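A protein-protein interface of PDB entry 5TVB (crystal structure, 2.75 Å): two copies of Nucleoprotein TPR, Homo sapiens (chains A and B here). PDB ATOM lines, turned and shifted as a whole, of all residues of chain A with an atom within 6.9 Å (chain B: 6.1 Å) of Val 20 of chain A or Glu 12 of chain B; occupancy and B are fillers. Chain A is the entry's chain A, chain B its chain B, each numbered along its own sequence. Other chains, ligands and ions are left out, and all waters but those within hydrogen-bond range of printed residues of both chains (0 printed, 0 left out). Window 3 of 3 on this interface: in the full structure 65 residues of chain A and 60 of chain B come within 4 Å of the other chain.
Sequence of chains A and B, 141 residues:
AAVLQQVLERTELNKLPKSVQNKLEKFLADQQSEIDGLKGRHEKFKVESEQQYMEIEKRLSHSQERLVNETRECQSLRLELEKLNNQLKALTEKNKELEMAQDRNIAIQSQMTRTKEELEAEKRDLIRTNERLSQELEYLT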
ATOM      1  N   LEU A   4      24.922   6.356  17.310  1.00  0.00           N
ATOM      2  CA  LEU A   4      24.223   6.479  18.591  1.00  0.00           C
ATOM      3  C   LEU A   4      22.718   6.282  18.480  1.00  0.00           C
ATOM      4  O   LEU A   4      22.072   5.863  19.441  1.00  0.00           O
ATOM      5  CB  LEU A   4      24.517   7.833  19.239  1.00  0.00           C
ATOM      6  CG  LEU A   4      25.670   7.821  20.247  1.00  0.00           C
ATOM      7  CD1 LEU A   4      25.762   9.147  20.983  1.00  0.00           C
ATOM      8  CD2 LEU A   4      25.517   6.669  21.230  1.00  0.00           C
ATOM      9  N   LEU A  16      21.653  13.860  26.159  1.00  0.00           N
ATOM     10  CA  LEU A  16      23.110  13.857  26.153  1.00  0.00           C
ATOM     11  C   LEU A  16      23.633  15.165  25.583  1.00  0.00           C
ATOM     12  O   LEU A  16      23.247  15.559  24.483  1.00  0.00           O
ATOM     13  CB  LEU A  16      23.658  12.687  25.332  1.00  0.00           C
ATOM     14  CG  LEU A  16      23.175  11.271  25.638  1.00  0.00           C
ATOM     15  CD1 LEU A  16      23.945  10.264  24.799  1.00  0.00           C
ATOM     16  CD2 LEU A  16      23.319  10.962  27.112  1.00  0.00           C
ATOM     17  N   PRO A  17      24.521  15.840  26.327  1.00  0.00           N
ATOM     18  CA  PRO A  17      25.193  17.049  25.844  1.00  0.00           C
ATOM     19  C   PRO A  17      25.956  16.798  24.546  1.00  0.00           C
ATOM     20  O   PRO A  17      26.405  15.676  24.311  1.00  0.00           O
ATOM     21  CB  PRO A  17      26.146  17.401  26.988  1.00  0.00           C
ATOM     22  CG  PRO A  17      25.503  16.821  28.197  1.00  0.00           C
ATOM     23  CD  PRO A  17      24.841  15.554  27.736  1.00  0.00           C
ATOM     24  N   LYS A  18      26.088  17.833  23.721  1.00  0.00           N
ATOM     25  CA  LYS A  18      26.713  17.721  22.406  1.00  0.00           C
ATOM     26  C   LYS A  18      28.127  17.158  22.495  1.00  0.00           C
ATOM     27  O   LYS A  18      28.518  16.313  21.690  1.00  0.00           O
ATOM     28  CB  LYS A  18      26.750  19.093  21.731  1.00  0.00           C
ATOM     29  CG  LYS A  18      26.661  19.089  20.217  1.00  0.00           C
ATOM     30  CD  LYS A  18      26.784  20.514  19.694  1.00  0.00           C
ATOM     31  CE  LYS A  18      26.645  20.587  18.185  1.00  0.00           C
ATOM     32  NZ  LYS A  18      26.920  21.965  17.686  1.00  0.00           N
ATOM     33  N   SER A  19      28.881  17.630  23.481  1.00  0.00           N
ATOM     34  CA  SER A  19      30.236  17.147  23.717  1.00  0.00           C
ATOM     35  C   SER A  19      30.244  15.652  24.011  1.00  0.00           C
ATOM     36  O   SER A  19      31.066  14.906  23.478  1.00  0.00           O
ATOM     37  CB  SER A  19      30.885  17.914  24.871  1.00  0.00           C
ATOM     38  OG  SER A  19      30.043  17.924  26.011  1.00  0.00           O
ATOM     39  N   VAL A  20      29.319  15.227  24.864  1.00  0.00           N
ATOM     40  CA  VAL A  20      29.191  13.822  25.230  1.00  0.00           C
ATOM     41  C   VAL A  20      28.891  12.946  24.017  1.00  0.00           C
ATOM     42  O   VAL A  20      29.472  11.872  23.862  1.00  0.00           O
ATOM     43  CB  VAL A  20      28.090  13.623  26.287  1.00  0.00           C
ATOM     44  CG1 VAL A  20      27.876  12.144  26.565  1.00  0.00           C
ATOM     45  CG2 VAL A  20      28.451  14.358  27.564  1.00  0.00           C
ATOM     46  N   GLN A  21      27.991  13.408  23.155  1.00  0.00           N
ATOM     47  CA  GLN A  21      27.661  12.655  21.951  1.00  0.00           C
ATOM     48  C   GLN A  21      28.857  12.594  21.011  1.00  0.00           C
ATOM     49  O   GLN A  21      29.149  11.549  20.436  1.00  0.00           O
ATOM     50  CB  GLN A  21      26.462  13.266  21.225  1.00  0.00           C
ATOM     51  CG  GLN A  21      25.161  13.234  22.007  1.00  0.00           C
ATOM     52  CD  GLN A  21      23.998  13.803  21.215  1.00  0.00           C
ATOM     53  OE1 GLN A  21      24.023  13.825  19.983  1.00  0.00           O
ATOM     54  NE2 GLN A  21      22.971  14.267  21.918  1.00  0.00           N
ATOM     55  N   ASN A  22      29.556  13.717  20.870  1.00  0.00           N
ATOM     56  CA  ASN A  22      30.706  13.792  19.980  1.00  0.00           C
ATOM     57  C   ASN A  22      31.856  12.903  20.441  1.00  0.00           C
ATOM     58  O   ASN A  22      32.478  12.217  19.628  1.00  0.00           O
ATOM     59  CB  ASN A  22      31.179  15.238  19.842  1.00  0.00           C
ATOM     60  CG  ASN A  22      30.176  16.106  19.111  1.00  0.00           C
ATOM     61  OD1 ASN A  22      29.196  15.608  18.558  1.00  0.00           O
ATOM     62  ND2 ASN A  22      30.416  17.413  19.102  1.00  0.00           N
ATOM     63  N   LYS A  23      32.140  12.918  21.740  1.00  0.00           N
ATOM     64  CA  LYS A  23      33.145  12.024  22.306  1.00  0.00           C
ATOM     65  C   LYS A  23      32.763  10.570  22.056  1.00  0.00           C
ATOM     66  O   LYS A  23      33.598   9.751  21.673  1.00  0.00           O
ATOM     67  CB  LYS A  23      33.302  12.258  23.812  1.00  0.00           C
ATOM     68  CG  LYS A  23      33.991  13.552  24.205  1.00  0.00           C
ATOM     69  CD  LYS A  23      34.430  13.491  25.662  1.00  0.00           C
ATOM     70  CE  LYS A  23      34.911  14.842  26.170  1.00  0.00           C
ATOM     71  NZ  LYS A  23      35.218  14.796  27.631  1.00  0.00           N
ATOM     72  N   LEU A  24      31.488  10.261  22.268  1.00  0.00           N
ATOM     73  CA  LEU A  24      30.969   8.917  22.043  1.00  0.00           C
ATOM     74  C   LEU A  24      30.969   8.534  20.568  1.00  0.00           C
ATOM     75  O   LEU A  24      31.353   7.418  20.210  1.00  0.00           O
ATOM     76  CB  LEU A  24      29.552   8.793  22.603  1.00  0.00           C
ATOM     77  CG  LEU A  24      29.411   8.603  24.114  1.00  0.00           C
ATOM     78  CD1 LEU A  24      27.944   8.498  24.504  1.00  0.00           C
ATOM     79  CD2 LEU A  24      30.176   7.373  24.572  1.00  0.00           C
ATOM     80  N   GLU A  25      30.534   9.459  19.718  1.00  0.00           N
ATOM     81  CA  GLU A  25      30.467   9.205  18.284  1.00  0.00           C
ATOM     82  C   GLU A  25      31.831   8.836  17.726  1.00  0.00           C
ATOM     83  O   GLU A  25      31.971   7.851  17.001  1.00  0.00           O
ATOM     84  CB  GLU A  25      29.926  10.428  17.540  1.00  0.00           C
ATOM     85  CG  GLU A  25      28.407  10.543  17.510  1.00  0.00           C
ATOM     86  CD  GLU A  25      27.723   9.340  16.886  1.00  0.00           C
ATOM     87  OE1 GLU A  25      28.360   8.628  16.080  1.00  0.00           O
ATOM     88  OE2 GLU A  25      26.535   9.114  17.198  1.00  0.00           O
ATOM     89  N   VAL B   7      35.970   6.785  27.445  1.00  0.00           N
ATOM     90  CA  VAL B   7      35.438   7.896  26.669  1.00  0.00           C
ATOM     91  C   VAL B   7      35.101   9.167  27.469  1.00  0.00           C
ATOM     92  O   VAL B   7      35.438  10.268  27.035  1.00  0.00           O
ATOM     93  CB  VAL B   7      34.176   7.452  25.910  1.00  0.00           C
ATOM     94  CG1 VAL B   7      33.859   8.445  24.807  1.00  0.00           C
ATOM     95  CG2 VAL B   7      34.391   6.071  25.315  1.00  0.00           C
ATOM     96  N   LEU B   8      34.430   9.032  28.612  1.00  0.00           N
ATOM     97  CA  LEU B   8      33.972  10.214  29.351  1.00  0.00           C
ATOM     98  C   LEU B   8      34.597  10.363  30.741  1.00  0.00           C
ATOM     99  O   LEU B   8      34.990   9.380  31.366  1.00  0.00           O
ATOM    100  CB  LEU B   8      32.454  10.157  29.511  1.00  0.00           C
ATOM    101  CG  LEU B   8      31.599   9.508  28.420  1.00  0.00           C
ATOM    102  CD1 LEU B   8      30.247   9.199  29.018  1.00  0.00           C
ATOM    103  CD2 LEU B   8      31.419  10.409  27.207  1.00  0.00           C
ATOM    104  N   GLU B   9      34.592  11.591  31.251  1.00  0.00           N
ATOM    105  CA  GLU B   9      35.099  11.897  32.586  1.00  0.00           C
ATOM    106  C   GLU B   9      34.031  11.693  33.665  1.00  0.00           C
ATOM    107  O   GLU B   9      32.834  11.757  33.386  1.00  0.00           O
ATOM    108  CB  GLU B   9      35.664  13.321  32.616  1.00  0.00           C
ATOM    109  CG  GLU B   9      34.677  14.418  32.272  1.00  0.00           C
ATOM    110  CD  GLU B   9      35.373  15.735  31.989  1.00  0.00           C
ATOM    111  OE1 GLU B   9      36.618  15.781  32.088  1.00  0.00           O
ATOM    112  OE2 GLU B   9      34.680  16.727  31.677  1.00  0.00           O
ATOM    113  N   ARG B  10      34.490  11.464  34.895  1.00  0.00           N
ATOM    114  CA  ARG B  10      33.651  11.097  36.040  1.00  0.00           C
ATOM    115  C   ARG B  10      32.357  11.900  36.191  1.00  0.00           C
ATOM    116  O   ARG B  10      31.300  11.333  36.470  1.00  0.00           O
ATOM    117  CB  ARG B  10      34.482  11.232  37.319  1.00  0.00           C
ATOM    118  CG  ARG B  10      33.692  11.183  38.610  1.00  0.00           C
ATOM    119  CD  ARG B  10      34.620  11.294  39.807  1.00  0.00           C
ATOM    120  NE  ARG B  10      35.594  10.207  39.845  1.00  0.00           N
ATOM    121  CZ  ARG B  10      36.892  10.355  39.603  1.00  0.00           C
ATOM    122  NH1 ARG B  10      37.703   9.308  39.657  1.00  0.00           N
ATOM    123  NH2 ARG B  10      37.381  11.552  39.312  1.00  0.00           N
ATOM    124  N   THR B  11      32.440  13.212  36.001  1.00  0.00           N
ATOM    125  CA  THR B  11      31.267  14.077  36.100  1.00  0.00           C
ATOM    126  C   THR B  11      30.213  13.727  35.053  1.00  0.00           C
ATOM    127  O   THR B  11      29.030  13.588  35.366  1.00  0.00           O
ATOM    128  CB  THR B  11      31.646  15.559  35.944  1.00  0.00           C
ATOM    129  OG1 THR B  11      32.616  15.910  36.938  1.00  0.00           O
ATOM    130  CG2 THR B  11      30.417  16.441  36.107  1.00  0.00           C
ATOM    131  N   GLU B  12      30.662  13.586  33.811  1.00  0.00           N
ATOM    132  CA  GLU B  12      29.790  13.290  32.679  1.00  0.00           C
ATOM    133  C   GLU B  12      28.999  11.995  32.856  1.00  0.00           C
ATOM    134  O   GLU B  12      27.810  11.937  32.546  1.00  0.00           O
ATOM    135  CB  GLU B  12      30.626  13.214  31.400  1.00  0.00           C
ATOM    136  CG  GLU B  12      30.841  14.550  30.716  1.00  0.00           C
ATOM    137  CD  GLU B  12      31.995  14.518  29.732  1.00  0.00           C
ATOM    138  OE1 GLU B  12      32.513  13.416  29.447  1.00  0.00           O
ATOM    139  OE2 GLU B  12      32.386  15.598  29.241  1.00  0.00           O
ATOM    140  N   LEU B  13      29.665  10.963  33.359  1.00  0.00           N
ATOM    141  CA  LEU B  13      29.082   9.633  33.458  1.00  0.00           C
ATOM    142  C   LEU B  13      27.945   9.565  34.489  1.00  0.00           C
ATOM    143  O   LEU B  13      27.012   8.770  34.323  1.00  0.00           O
ATOM    144  CB  LEU B  13      30.178   8.623  33.797  1.00  0.00           C
ATOM    145  CG  LEU B  13      29.755   7.169  33.922  1.00  0.00           C
ATOM    146  CD1 LEU B  13      29.063   6.833  32.660  1.00  0.00           C
ATOM    147  CD2 LEU B  13      30.966   6.283  34.135  1.00  0.00           C
ATOM    148  N   ASN B  14      28.027  10.405  35.531  1.00  0.00           N
ATOM    149  CA  ASN B  14      27.043  10.439  36.624  1.00  0.00           C
ATOM    150  C   ASN B  14      25.745  11.171  36.283  1.00  0.00           C
ATOM    151  O   ASN B  14      24.774  11.108  37.039  1.00  0.00           O
ATOM    152  CB  ASN B  14      27.650  11.084  37.877  1.00  0.00           C
ATOM    153  CG  ASN B  14      28.713  10.220  38.528  1.00  0.00           C
ATOM    154  OD1 ASN B  14      28.808   9.022  38.259  1.00  0.00           O
ATOM    155  ND2 ASN B  14      29.514  10.824  39.398  1.00  0.00           N
ATOM    156  N   LYS B  15      25.724  11.864  35.150  1.00  0.00           N
ATOM    157  CA  LYS B  15      24.505  12.534  34.713  1.00  0.00           C
ATOM    158  C   LYS B  15      23.706  11.618  33.797  1.00  0.00           C
ATOM    159  O   LYS B  15      22.631  11.978  33.321  1.00  0.00           O
ATOM    160  CB  LYS B  15      24.823  13.853  34.008  1.00  0.00           C
ATOM    161  CG  LYS B  15      25.658  14.814  34.838  1.00  0.00           C
ATOM    162  CD  LYS B  15      25.300  16.255  34.517  1.00  0.00           C
ATOM    163  CE  LYS B  15      23.867  16.552  34.935  1.00  0.00           C
ATOM    164  NZ  LYS B  15      23.483  17.970  34.695  1.00  0.00           N
ATOM    165  N   LEU B  16      24.246  10.428  33.564  1.00  0.00           N
ATOM    166  CA  LEU B  16      23.598   9.436  32.716  1.00  0.00           C
ATOM    167  C   LEU B  16      22.800   8.443  33.548  1.00  0.00           C
ATOM    168  O   LEU B  16      23.321   7.891  34.517  1.00  0.00           O
ATOM    169  CB  LEU B  16      24.636   8.686  31.880  1.00  0.00           C
ATOM    170  CG  LEU B  16      25.626   9.526  31.074  1.00  0.00           C
ATOM    171  CD1 LEU B  16      26.498   8.634  30.203  1.00  0.00           C
ATOM    172  CD2 LEU B  16      24.898  10.558  30.240  1.00  0.00           C
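The side-chain carboxylate of Glu 12 of chain B is in salt-bridge range of the side-chain amino group of Lys 23 of chain A, at 3.4 Å.
The backbone carbonyl oxygen (O) of Leu 16 of chain A sits at hydrogen-bond distance from the side-chain amide nitrogen (NE2) of Gln 21 of chain A.
The backbone NH (N) of Glu 9 of chain B sits at hydrogen-bond distance from the side-chain carboxylate (OE1) of Glu 12 of chain B, 3.3 Å away.
Leu 16 of chain B touches Leu 16 of chain A.
Leu 8 of chain B touches Val 20 of chain A (CD2 to CG1, 3.997 Å).
Val 20 of chain A touches Glu 12 of chain B.
Lys 23 of chain A touches Val 7 of chain B.
CD2 of Leu 24 of chain A touches CG1 of Val 7 of chain B, 3.8 Å away.
Printed residues of chain B within 4 Å of Leu 16 of chain A: Leu 16 (3.5 Å).
Of the printed residues of chain B, Val 20 of chain A touches Leu 8 (3.997 Å) and Glu 12 (3.96 Å).
Of the printed residues of chain B, Leu 24 of chain A touches Val 7.
Of the printed residues of chain A, Val 7 of chain B touches Lys 23 (3.4 Å) and Leu 24 (3.8 Å).
Printed residues of chain A within 4 Å of Leu 8 of chain B: Val 20 (3.997 Å).
Of the printed residues of chain A, Glu 12 of chain B touches Val 20 (3.96 Å) and Lys 23 (3.4 Å).
Of the printed residues of chain A, Leu 16 of chain B touches Leu 16 (3.5 Å).
The nearest residue of chain A that does not touch Glu 12 of chain B is Ser 19 of chain A (4.6 Å).
Hydrophobic or aromatic side chains of chain A within 4 Å of the printed part of chain B: Leu 16, Val 20 and Leu 24.
Among the printed residues, Asp or Glu carboxylates within 4 Å of a Lys or Arg side-chain nitrogen of the other chain: Lys 23 of chain A with Glu 12 of chain B (3.4 Å).
Leu 16 of chain B touches its own counterpart, Leu 16 of chain A.
1 position is printed for both chains.
Of the 6 pairs that touch across the chains among the printed residues, 1 has its exchanged pair printed and touching as well.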
